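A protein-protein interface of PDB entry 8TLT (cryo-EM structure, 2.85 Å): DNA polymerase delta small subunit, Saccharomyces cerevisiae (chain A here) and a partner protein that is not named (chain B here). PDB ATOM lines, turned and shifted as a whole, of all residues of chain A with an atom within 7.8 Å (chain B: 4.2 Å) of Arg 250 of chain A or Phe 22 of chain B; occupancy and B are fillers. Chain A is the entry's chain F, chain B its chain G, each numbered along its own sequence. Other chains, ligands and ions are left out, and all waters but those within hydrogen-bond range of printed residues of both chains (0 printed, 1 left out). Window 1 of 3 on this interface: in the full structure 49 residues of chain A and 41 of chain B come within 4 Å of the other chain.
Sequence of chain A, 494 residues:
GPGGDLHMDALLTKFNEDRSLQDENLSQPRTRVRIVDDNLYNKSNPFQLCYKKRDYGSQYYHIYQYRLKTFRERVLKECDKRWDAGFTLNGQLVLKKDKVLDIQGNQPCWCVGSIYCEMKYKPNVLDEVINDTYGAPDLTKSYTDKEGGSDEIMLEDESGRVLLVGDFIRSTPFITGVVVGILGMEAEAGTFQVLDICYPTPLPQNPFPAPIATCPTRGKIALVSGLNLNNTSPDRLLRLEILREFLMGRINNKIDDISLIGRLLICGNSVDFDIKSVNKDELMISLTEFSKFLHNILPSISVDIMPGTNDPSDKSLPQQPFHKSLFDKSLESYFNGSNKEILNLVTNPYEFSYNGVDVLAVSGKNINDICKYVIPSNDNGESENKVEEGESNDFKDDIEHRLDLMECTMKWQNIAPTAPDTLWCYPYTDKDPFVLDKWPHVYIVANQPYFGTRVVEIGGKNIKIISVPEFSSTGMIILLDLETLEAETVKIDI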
ATOM      1  N   LEU A  26     -14.214 -18.802   5.796  1.00  0.00           N
ATOM      2  CA  LEU A  26     -13.082 -17.905   6.015  1.00  0.00           C
ATOM      3  C   LEU A  26     -13.476 -16.608   6.710  1.00  0.00           C
ATOM      4  O   LEU A  26     -12.599 -15.777   6.974  1.00  0.00           O
ATOM      5  CB  LEU A  26     -12.343 -17.565   4.712  1.00  0.00           C
ATOM      6  CG  LEU A  26     -10.853 -17.906   4.662  1.00  0.00           C
ATOM      7  N   ILE A 242       5.677 -26.454   0.988  1.00  0.00           N
ATOM      8  CA  ILE A 242       4.640 -27.477   1.096  1.00  0.00           C
ATOM      9  C   ILE A 242       4.339 -27.779   2.559  1.00  0.00           C
ATOM     10  O   ILE A 242       3.177 -27.968   2.939  1.00  0.00           O
ATOM     11  CB  ILE A 242       5.050 -28.742   0.323  1.00  0.00           C
ATOM     12  CG1 ILE A 242       5.143 -28.441  -1.174  1.00  0.00           C
ATOM     13  CG2 ILE A 242       4.056 -29.865   0.574  1.00  0.00           C
ATOM     14  CD1 ILE A 242       5.129 -29.670  -2.054  1.00  0.00           C
ATOM     15  N   ARG A 244       4.679 -25.651   5.061  1.00  0.00           N
ATOM     16  CA  ARG A 244       3.934 -24.506   5.574  1.00  0.00           C
ATOM     17  C   ARG A 244       2.474 -24.567   5.150  1.00  0.00           C
ATOM     18  O   ARG A 244       1.575 -24.300   5.954  1.00  0.00           O
ATOM     19  CB  ARG A 244       4.573 -23.202   5.097  1.00  0.00           C
ATOM     20  CG  ARG A 244       3.688 -21.983   5.280  1.00  0.00           C
ATOM     21  CD  ARG A 244       4.400 -20.710   4.867  1.00  0.00           C
ATOM     22  NE  ARG A 244       4.246 -20.435   3.445  1.00  0.00           N
ATOM     23  CZ  ARG A 244       3.162 -19.903   2.897  1.00  0.00           C
ATOM     24  NH1 ARG A 244       2.109 -19.577   3.626  1.00  0.00           N
ATOM     25  NH2 ARG A 244       3.135 -19.694   1.584  1.00  0.00           N
ATOM     26  N   GLU A 245       2.219 -24.923   3.889  1.00  0.00           N
ATOM     27  CA  GLU A 245       0.842 -25.039   3.421  1.00  0.00           C
ATOM     28  C   GLU A 245       0.103 -26.158   4.143  1.00  0.00           C
ATOM     29  O   GLU A 245      -1.083 -26.022   4.465  1.00  0.00           O
ATOM     30  CB  GLU A 245       0.818 -25.262   1.910  1.00  0.00           C
ATOM     31  CG  GLU A 245       0.924 -23.982   1.097  1.00  0.00           C
ATOM     32  CD  GLU A 245       0.393 -22.774   1.842  1.00  0.00           C
ATOM     33  N   PHE A 246       0.785 -27.278   4.400  1.00  0.00           N
ATOM     34  CA  PHE A 246       0.156 -28.381   5.119  1.00  0.00           C
ATOM     35  C   PHE A 246      -0.200 -27.984   6.544  1.00  0.00           C
ATOM     36  O   PHE A 246      -1.285 -28.315   7.036  1.00  0.00           O
ATOM     37  CB  PHE A 246       1.077 -29.601   5.120  1.00  0.00           C
ATOM     38  CG  PHE A 246       0.755 -30.602   6.194  1.00  0.00           C
ATOM     39  CD1 PHE A 246      -0.327 -31.456   6.061  1.00  0.00           C
ATOM     40  CD2 PHE A 246       1.533 -30.691   7.336  1.00  0.00           C
ATOM     41  CE1 PHE A 246      -0.627 -32.376   7.045  1.00  0.00           C
ATOM     42  CE2 PHE A 246       1.235 -31.608   8.324  1.00  0.00           C
ATOM     43  CZ  PHE A 246       0.156 -32.452   8.178  1.00  0.00           C
ATOM     44  N   LEU A 247       0.704 -27.278   7.227  1.00  0.00           N
ATOM     45  CA  LEU A 247       0.452 -26.881   8.607  1.00  0.00           C
ATOM     46  C   LEU A 247      -0.675 -25.865   8.724  1.00  0.00           C
ATOM     47  O   LEU A 247      -1.272 -25.741   9.799  1.00  0.00           O
ATOM     48  CB  LEU A 247       1.727 -26.315   9.233  1.00  0.00           C
ATOM     49  CG  LEU A 247       2.790 -27.333   9.646  1.00  0.00           C
ATOM     50  CD1 LEU A 247       3.990 -26.634  10.261  1.00  0.00           C
ATOM     51  CD2 LEU A 247       2.210 -28.354  10.611  1.00  0.00           C
ATOM     52  N   MET A 248      -0.982 -25.139   7.652  1.00  0.00           N
ATOM     53  CA  MET A 248      -2.050 -24.150   7.654  1.00  0.00           C
ATOM     54  C   MET A 248      -3.394 -24.727   7.226  1.00  0.00           C
ATOM     55  O   MET A 248      -4.387 -23.994   7.212  1.00  0.00           O
ATOM     56  CB  MET A 248      -1.682 -22.976   6.743  1.00  0.00           C
ATOM     57  CG  MET A 248      -0.452 -22.206   7.192  1.00  0.00           C
ATOM     58  SD  MET A 248      -0.316 -20.584   6.419  1.00  0.00           S
ATOM     59  N   GLY A 249      -3.450 -26.010   6.882  1.00  0.00           N
ATOM     60  CA  GLY A 249      -4.684 -26.641   6.468  1.00  0.00           C
ATOM     61  C   GLY A 249      -5.034 -26.499   5.005  1.00  0.00           C
ATOM     62  O   GLY A 249      -6.136 -26.900   4.610  1.00  0.00           O
ATOM     63  N   ARG A 250      -4.141 -25.941   4.186  1.00  0.00           N
ATOM     64  CA  ARG A 250      -4.435 -25.778   2.765  1.00  0.00           C
ATOM     65  C   ARG A 250      -4.296 -27.089   2.000  1.00  0.00           C
ATOM     66  O   ARG A 250      -5.050 -27.339   1.054  1.00  0.00           O
ATOM     67  CB  ARG A 250      -3.522 -24.714   2.158  1.00  0.00           C
ATOM     68  CG  ARG A 250      -3.346 -23.475   3.014  1.00  0.00           C
ATOM     69  CD  ARG A 250      -4.410 -22.442   2.706  1.00  0.00           C
ATOM     70  NE  ARG A 250      -4.357 -21.313   3.626  1.00  0.00           N
ATOM     71  CZ  ARG A 250      -3.517 -20.295   3.513  1.00  0.00           C
ATOM     72  NH1 ARG A 250      -2.634 -20.232   2.531  1.00  0.00           N
ATOM     73  NH2 ARG A 250      -3.565 -19.312   4.408  1.00  0.00           N
ATOM     74  N   ILE A 251      -3.343 -27.934   2.388  1.00  0.00           N
ATOM     75  CA  ILE A 251      -3.049 -29.153   1.643  1.00  0.00           C
ATOM     76  C   ILE A 251      -3.956 -30.286   2.103  1.00  0.00           C
ATOM     77  O   ILE A 251      -4.676 -30.884   1.296  1.00  0.00           O
ATOM     78  CB  ILE A 251      -1.566 -29.544   1.786  1.00  0.00           C
ATOM     79  CG1 ILE A 251      -0.682 -28.569   1.007  1.00  0.00           C
ATOM     80  CG2 ILE A 251      -1.340 -30.965   1.305  1.00  0.00           C
ATOM     81  N   ASN A 252      -3.925 -30.592   3.402  1.00  0.00           N
ATOM     82  CA  ASN A 252      -4.726 -31.696   3.921  1.00  0.00           C
ATOM     83  C   ASN A 252      -6.218 -31.409   3.797  1.00  0.00           C
ATOM     84  O   ASN A 252      -7.006 -32.315   3.503  1.00  0.00           O
ATOM     85  CB  ASN A 252      -4.354 -31.977   5.377  1.00  0.00           C
ATOM     86  CG  ASN A 252      -4.772 -33.360   5.827  1.00  0.00           C
ATOM     87  OD1 ASN A 252      -5.960 -33.671   5.891  1.00  0.00           O
ATOM     88  ND2 ASN A 252      -3.794 -34.200   6.142  1.00  0.00           N
ATOM     89  N   ASN A 253      -6.623 -30.162   4.040  1.00  0.00           N
ATOM     90  CA  ASN A 253      -7.996 -29.667   3.968  1.00  0.00           C
ATOM     91  C   ASN A 253      -8.899 -30.251   5.045  1.00  0.00           C
ATOM     92  O   ASN A 253     -10.081 -29.889   5.101  1.00  0.00           O
ATOM     93  CB  ASN A 253      -8.642 -29.914   2.596  1.00  0.00           C
ATOM     94  CG  ASN A 253      -8.498 -28.731   1.663  1.00  0.00           C
ATOM     95  OD1 ASN A 253      -7.825 -27.752   1.983  1.00  0.00           O
ATOM     96  ND2 ASN A 253      -9.133 -28.815   0.501  1.00  0.00           N
ATOM     97  N   LYS A 254      -8.394 -31.138   5.904  1.00  0.00           N
ATOM     98  CA  LYS A 254      -9.165 -31.639   7.040  1.00  0.00           C
ATOM     99  C   LYS A 254      -8.907 -30.708   8.221  1.00  0.00           C
ATOM    100  O   LYS A 254      -8.068 -30.956   9.088  1.00  0.00           O
ATOM    101  CB  LYS A 254      -8.796 -33.083   7.352  1.00  0.00           C
ATOM    102  CG  LYS A 254      -9.714 -33.753   8.361  1.00  0.00           C
ATOM    103  CD  LYS A 254      -9.398 -35.231   8.501  1.00  0.00           C
ATOM    104  N   ILE A 255      -9.657 -29.603   8.239  1.00  0.00           N
ATOM    105  CA  ILE A 255      -9.459 -28.544   9.223  1.00  0.00           C
ATOM    106  C   ILE A 255      -9.686 -28.997  10.656  1.00  0.00           C
ATOM    107  O   ILE A 255      -9.222 -28.327  11.585  1.00  0.00           O
ATOM    108  CB  ILE A 255     -10.365 -27.347   8.867  1.00  0.00           C
ATOM    109  CG1 ILE A 255     -11.850 -27.733   8.931  1.00  0.00           C
ATOM    110  CG2 ILE A 255     -10.013 -26.807   7.489  1.00  0.00           C
ATOM    111  CD1 ILE A 255     -12.541 -27.449  10.249  1.00  0.00           C
ATOM    112  N   ILE A 258      -6.103 -30.812  11.490  1.00  0.00           N
ATOM    113  CA  ILE A 258      -4.965 -29.905  11.363  1.00  0.00           C
ATOM    114  C   ILE A 258      -4.970 -28.869  12.480  1.00  0.00           C
ATOM    115  O   ILE A 258      -3.907 -28.467  12.969  1.00  0.00           O
ATOM    116  CB  ILE A 258      -4.966 -29.250   9.969  1.00  0.00           C
ATOM    117  CG1 ILE A 258      -4.594 -30.279   8.902  1.00  0.00           C
ATOM    118  CG2 ILE A 258      -3.996 -28.082   9.917  1.00  0.00           C
ATOM    119  N   ASN A 296       5.279 -15.791   6.737  1.00  0.00           N
ATOM    120  CA  ASN A 296       4.091 -16.362   6.114  1.00  0.00           C
ATOM    121  C   ASN A 296       3.398 -17.374   7.019  1.00  0.00           C
ATOM    122  O   ASN A 296       2.186 -17.583   6.888  1.00  0.00           O
ATOM    123  CB  ASN A 296       4.458 -17.008   4.779  1.00  0.00           C
ATOM    124  CG  ASN A 296       4.733 -15.988   3.697  1.00  0.00           C
ATOM    125  OD1 ASN A 296       4.289 -14.844   3.780  1.00  0.00           O
ATOM    126  ND2 ASN A 296       5.467 -16.398   2.671  1.00  0.00           N
ATOM    127  N   SER A 300      -0.548 -18.115  11.511  1.00  0.00           N
ATOM    128  CA  SER A 300      -1.404 -19.284  11.663  1.00  0.00           C
ATOM    129  C   SER A 300      -0.981 -20.211  12.792  1.00  0.00           C
ATOM    130  O   SER A 300      -1.838 -20.873  13.385  1.00  0.00           O
ATOM    131  CB  SER A 300      -1.448 -20.082  10.357  1.00  0.00           C
ATOM    132  OG  SER A 300      -2.680 -20.766  10.220  1.00  0.00           O
ATOM    133  N   LEU B  21      -0.082 -20.891  -8.453  1.00  0.00           N
ATOM    134  CA  LEU B  21      -0.471 -21.823  -7.407  1.00  0.00           C
ATOM    135  C   LEU B  21      -1.894 -21.528  -6.949  1.00  0.00           C
ATOM    136  O   LEU B  21      -2.406 -20.420  -7.114  1.00  0.00           O
ATOM    137  CB  LEU B  21       0.493 -21.737  -6.221  1.00  0.00           C
ATOM    138  CG  LEU B  21       1.838 -22.454  -6.360  1.00  0.00           C
ATOM    139  CD1 LEU B  21       2.876 -21.538  -6.980  1.00  0.00           C
ATOM    140  CD2 LEU B  21       2.314 -22.953  -5.011  1.00  0.00           C
ATOM    141  N   PHE B  22      -2.539 -22.545  -6.374  1.00  0.00           N
ATOM    142  CA  PHE B  22      -3.885 -22.344  -5.852  1.00  0.00           C
ATOM    143  C   PHE B  22      -3.888 -21.459  -4.612  1.00  0.00           C
ATOM    144  O   PHE B  22      -4.898 -20.798  -4.335  1.00  0.00           O
ATOM    145  CB  PHE B  22      -4.548 -23.693  -5.563  1.00  0.00           C
ATOM    146  CG  PHE B  22      -4.108 -24.333  -4.278  1.00  0.00           C
ATOM    147  CD1 PHE B  22      -2.856 -24.911  -4.167  1.00  0.00           C
ATOM    148  CD2 PHE B  22      -4.958 -24.375  -3.186  1.00  0.00           C
ATOM    149  CE1 PHE B  22      -2.454 -25.506  -2.988  1.00  0.00           C
ATOM    150  CE2 PHE B  22      -4.563 -24.967  -2.005  1.00  0.00           C
ATOM    151  CZ  PHE B  22      -3.309 -25.534  -1.906  1.00  0.00           C
ATOM    152  N   THR B  23      -2.778 -21.417  -3.872  1.00  0.00           N
ATOM    153  CA  THR B  23      -2.657 -20.455  -2.784  1.00  0.00           C
ATOM    154  C   THR B  23      -2.651 -19.025  -3.306  1.00  0.00           C
ATOM    155  O   THR B  23      -3.078 -18.106  -2.598  1.00  0.00           O
ATOM    156  CB  THR B  23      -1.393 -20.732  -1.972  1.00  0.00           C
ATOM    157  OG1 THR B  23      -0.309 -21.028  -2.859  1.00  0.00           O
ATOM    158  CG2 THR B  23      -1.612 -21.913  -1.045  1.00  0.00           C
ATOM    159  N   ASP B  24      -2.179 -18.814  -4.538  1.00  0.00           N
ATOM    160  CA  ASP B  24      -2.286 -17.494  -5.147  1.00  0.00           C
ATOM    161  C   ASP B  24      -3.744 -17.098  -5.338  1.00  0.00           C
ATOM    162  O   ASP B  24      -4.123 -15.954  -5.068  1.00  0.00           O
ATOM    163  CB  ASP B  24      -1.537 -17.461  -6.479  1.00  0.00           C
ATOM    164  CG  ASP B  24      -0.117 -17.976  -6.362  1.00  0.00           C
ATOM    165  N   LEU B  25      -4.583 -18.036  -5.791  1.00  0.00           N
ATOM    166  CA  LEU B  25      -6.015 -17.765  -5.873  1.00  0.00           C
ATOM    167  C   LEU B  25      -6.606 -17.519  -4.492  1.00  0.00           C
ATOM    168  O   LEU B  25      -7.475 -16.655  -4.325  1.00  0.00           O
ATOM    169  CB  LEU B  25      -6.739 -18.924  -6.556  1.00  0.00           C
ATOM    170  CG  LEU B  25      -6.442 -19.178  -8.032  1.00  0.00           C
ATOM    171  CD1 LEU B  25      -6.876 -20.582  -8.420  1.00  0.00           C
ATOM    172  CD2 LEU B  25      -7.128 -18.138  -8.901  1.00  0.00           C
ATOM    173  N   ILE B  26      -6.151 -18.278  -3.492  1.00  0.00           N
ATOM    174  CA  ILE B  26      -6.631 -18.088  -2.125  1.00  0.00           C
ATOM    175  C   ILE B  26      -6.350 -16.665  -1.660  1.00  0.00           C
ATOM    176  O   ILE B  26      -7.216 -15.995  -1.084  1.00  0.00           O
ATOM    177  CB  ILE B  26      -5.987 -19.122  -1.184  1.00  0.00           C
ATOM    178  CG1 ILE B  26      -6.561 -20.515  -1.440  1.00  0.00           C
ATOM    179  CG2 ILE B  26      -6.187 -18.725   0.268  1.00  0.00           C
ATOM    180  N   PRO B  33      -9.385 -22.989   0.582  1.00  0.00           N
ATOM    181  CA  PRO B  33      -8.542 -23.878  -0.237  1.00  0.00           C
ATOM    182  C   PRO B  33      -9.329 -24.864  -1.084  1.00  0.00           C
ATOM    183  O   PRO B  33      -8.911 -25.180  -2.205  1.00  0.00           O
ATOM    184  CB  PRO B  33      -7.669 -24.589   0.807  1.00  0.00           C
ATOM    185  CG  PRO B  33      -8.411 -24.453   2.092  1.00  0.00           C
ATOM    186  CD  PRO B  33      -9.122 -23.142   2.021  1.00  0.00           C
ATOM    187  N   ALA B  36     -10.493 -23.030  -4.049  1.00  0.00           N
ATOM    188  CA  ALA B  36      -9.353 -22.793  -4.930  1.00  0.00           C
ATOM    189  C   ALA B  36      -9.020 -24.036  -5.745  1.00  0.00           C
ATOM    190  O   ALA B  36      -8.725 -23.943  -6.943  1.00  0.00           O
ATOM    191  CB  ALA B  36      -8.142 -22.346  -4.115  1.00  0.00           C
ATOM    192  N   LYS B  37      -9.058 -25.209  -5.110  1.00  0.00           N
ATOM    193  CA  LYS B  37      -8.847 -26.454  -5.842  1.00  0.00           C
ATOM    194  C   LYS B  37      -9.932 -26.663  -6.889  1.00  0.00           C
ATOM    195  O   LYS B  37      -9.654 -27.131  -8.001  1.00  0.00           O
ATOM    196  CB  LYS B  37      -8.807 -27.631  -4.870  1.00  0.00           C
ATOM    197  CG  LYS B  37      -7.465 -27.837  -4.197  1.00  0.00           C
ATOM    198  CD  LYS B  37      -7.585 -28.786  -3.019  1.00  0.00           C
ATOM    199  CE  LYS B  37      -6.725 -28.335  -1.857  1.00  0.00           C
ATOM    200  NZ  LYS B  37      -6.251 -29.489  -1.049  1.00  0.00           N
ATOM    201  N   MET B  40      -9.137 -24.389  -9.791  1.00  0.00           N
ATOM    202  CA  MET B  40      -8.018 -24.944 -10.548  1.00  0.00           C
ATOM    203  C   MET B  40      -8.473 -26.097 -11.433  1.00  0.00           C
ATOM    204  O   MET B  40      -8.071 -26.193 -12.599  1.00  0.00           O
ATOM    205  CB  MET B  40      -6.912 -25.401  -9.598  1.00  0.00           C
ATOM    206  CG  MET B  40      -6.066 -24.276  -9.031  1.00  0.00           C
ATOM    207  SD  MET B  40      -4.445 -24.214  -9.822  1.00  0.00           S
ATOM    208  CE  MET B  40      -4.142 -22.453  -9.862  1.00  0.00           C
ATOM    209  N   PHE B  84      -5.403 -33.202  -6.324  1.00  0.00           N
ATOM    210  CA  PHE B  84      -5.762 -31.903  -6.872  1.00  0.00           C
ATOM    211  C   PHE B  84      -4.575 -31.319  -7.622  1.00  0.00           C
ATOM    212  O   PHE B  84      -3.437 -31.770  -7.473  1.00  0.00           O
ATOM    213  CB  PHE B  84      -6.223 -30.932  -5.780  1.00  0.00           C
ATOM    214  CG  PHE B  84      -5.181 -30.649  -4.734  1.00  0.00           C
ATOM    215  CD1 PHE B  84      -4.935 -31.555  -3.716  1.00  0.00           C
ATOM    216  CD2 PHE B  84      -4.445 -29.477  -4.771  1.00  0.00           C
ATOM    217  CE1 PHE B  84      -3.978 -31.294  -2.756  1.00  0.00           C
ATOM    218  CE2 PHE B  84      -3.489 -29.212  -3.812  1.00  0.00           C
ATOM    219  CZ  PHE B  84      -3.257 -30.120  -2.805  1.00  0.00           C
ATOM    220  N   TYR B  86      -1.891 -28.849  -7.935  1.00  0.00           N
ATOM    221  CA  TYR B  86      -1.178 -27.964  -7.020  1.00  0.00           C
ATOM    222  C   TYR B  86      -0.841 -26.635  -7.682  1.00  0.00           C
ATOM    223  O   TYR B  86      -1.010 -25.573  -7.072  1.00  0.00           O
ATOM    224  CB  TYR B  86       0.091 -28.646  -6.513  1.00  0.00           C
ATOM    225  CG  TYR B  86       0.902 -27.796  -5.563  1.00  0.00           C
ATOM    226  CD1 TYR B  86       0.321 -27.235  -4.436  1.00  0.00           C
ATOM    227  CD2 TYR B  86       2.250 -27.558  -5.794  1.00  0.00           C
ATOM    228  CE1 TYR B  86       1.058 -26.460  -3.564  1.00  0.00           C
ATOM    229  CE2 TYR B  86       2.994 -26.782  -4.928  1.00  0.00           C
ATOM    230  CZ  TYR B  86       2.394 -26.237  -3.815  1.00  0.00           C
ATOM    231  OH  TYR B  86       3.130 -25.464  -2.947  1.00  0.00           O
ATOM    232  N   GLN B 103      -1.548 -11.806   4.605  1.00  0.00           N
ATOM    233  CA  GLN B 103      -2.704 -12.670   4.848  1.00  0.00           C
ATOM    234  C   GLN B 103      -3.601 -12.035   5.910  1.00  0.00           C
ATOM    235  O   GLN B 103      -3.738 -12.513   7.038  1.00  0.00           O
ATOM    236  CB  GLN B 103      -2.246 -14.063   5.256  1.00  0.00           C
ATOM    237  CG  GLN B 103      -1.116 -14.613   4.404  1.00  0.00           C
ATOM    238  CD  GLN B 103      -0.954 -16.112   4.545  1.00  0.00           C
ATOM    239  OE1 GLN B 103      -1.833 -16.881   4.159  1.00  0.00           O
ATOM    240  NE2 GLN B 103       0.176 -16.534   5.095  1.00  0.00           N
ATOM    241  N   CYS B 106      -7.226 -14.078   4.724  1.00  0.00           N
ATOM    242  CA  CYS B 106      -7.204 -15.327   3.977  1.00  0.00           C
ATOM    243  C   CYS B 106      -6.947 -16.544   4.856  1.00  0.00           C
ATOM    244  O   CYS B 106      -6.900 -17.664   4.340  1.00  0.00           O
ATOM    245  CB  CYS B 106      -6.144 -15.259   2.872  1.00  0.00           C
ATOM    246  SG  CYS B 106      -5.888 -13.606   2.191  1.00  0.00           S
ATOM    247  N   THR B 108      -7.508 -19.673   7.207  1.00  0.00           N
ATOM    248  CA  THR B 108      -8.550 -20.638   7.531  1.00  0.00           C
ATOM    249  C   THR B 108      -8.370 -21.261   8.908  1.00  0.00           C
ATOM    250  O   THR B 108      -9.345 -21.770   9.472  1.00  0.00           O
ATOM    251  CB  THR B 108      -8.599 -21.748   6.473  1.00  0.00           C
ATOM    252  OG1 THR B 108      -9.619 -22.693   6.815  1.00  0.00           O
ATOM    253  CG2 THR B 108      -7.260 -22.461   6.381  1.00  0.00           C
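The side-chain amino group (NZ) of Lys 37 of chain B sits at hydrogen-bond distance from the backbone carbonyl oxygen (O) of Arg 250 of chain A, at 3.2 Å. The guanidinium group (NH2) of Arg 250 of chain A sits at hydrogen-bond distance from the side-chain amide oxygen (OE1) of Gln 103 of chain B. NZ of Lys 37 of chain B lies within hydrogen-bond range of O of Ile 251 of chain A (3.2 Å). The side-chain amide nitrogen (ND2) of Asn 253 of chain A sits close to the side-chain amino group (NZ) of Lys 37 of chain B (3.3 Å). NE2 of Gln 103 of chain B is in hydrogen-bond range of O of Asn 296 of chain A, at 2.9 Å.
Cys 106 of chain B touches Leu 26 of chain A (O to CG, 3.97 Å). NH1 of Arg 244 of chain A touches NE2 of Gln 103 of chain B, at 3.9 Å. Glu 245 of chain A touches Thr 23 of chain B (CD to CG2, 3.6 Å). Met 248 of chain A touches Thr 108 of chain B. Arg 250 of chain A touches Phe 22 of chain B (O to CZ, 3.9 Å). O of Arg 250 of chain A touches CB of Pro 33 of chain B, 3.8 Å away. Arg 250 of chain A touches Cys 106 of chain B. OD1 of Asn 253 of chain A touches CG of Pro 33 of chain B (3.4 Å).
The backbone NH (N) of Arg 250 of chain A sits at hydrogen-bond distance from the backbone carbonyl oxygen (O) of Glu 245 of chain A, 3.1 Å away. O of Gly 249 of chain A sits close to OD1 of Asn 253 of chain A, at 3.2 Å. The side-chain amide oxygen (OD1) of Asn 253 of chain A lies close to the backbone carbonyl oxygen (O) of Arg 250 of chain A (3.0 Å). The backbone NH (N) of Phe 22 of chain B lies within hydrogen-bond range of the backbone carbonyl oxygen (O) of Tyr 86 of chain B (3.5 Å).
Of the 17 printed residues of chain A, 8 touch a printed residue of chain B. Hydrophobic or aromatic side chains of chain A within 4 Å of the printed part of chain B: Leu 26. Of the 15 printed residues of chain B, 7 touch a printed residue of chain A. Printed residues of chain B that touch a printed residue of chain A: Phe 22, Thr 23, Pro 33, Lys 37, Gln 103, Cys 106 and Thr 108. Among the printed residues, no Asp or Glu carboxylate lies within 4 Å of a Lys or Arg side-chain nitrogen of the other chain.
Arg 250 of chain A touches just these residues of chain B: Phe 22, Pro 33, Lys 37, Gln 103 and Cys 106. Phe 22 of chain B touches just one residue of chain A: Arg 250 (3.9 Å). Printed residues of chain A within 4 Å of Thr 23 of chain B: Glu 245. Printed residues of chain B within 4 Å of Asn 296 of chain A: Gln 103 (2.9 Å). Asn 252 of chain A touches none of the printed residues of chain B. Ile 242 of chain A touches none of the printed residues of chain B. The nearest residue of chain A that does not touch Phe 22 of chain B is Ile 251 of chain A (4.9 Å). The nearest printed residue of chain B that does not touch Asn 253 of chain A is Phe 22 of chain B (5.9 Å).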
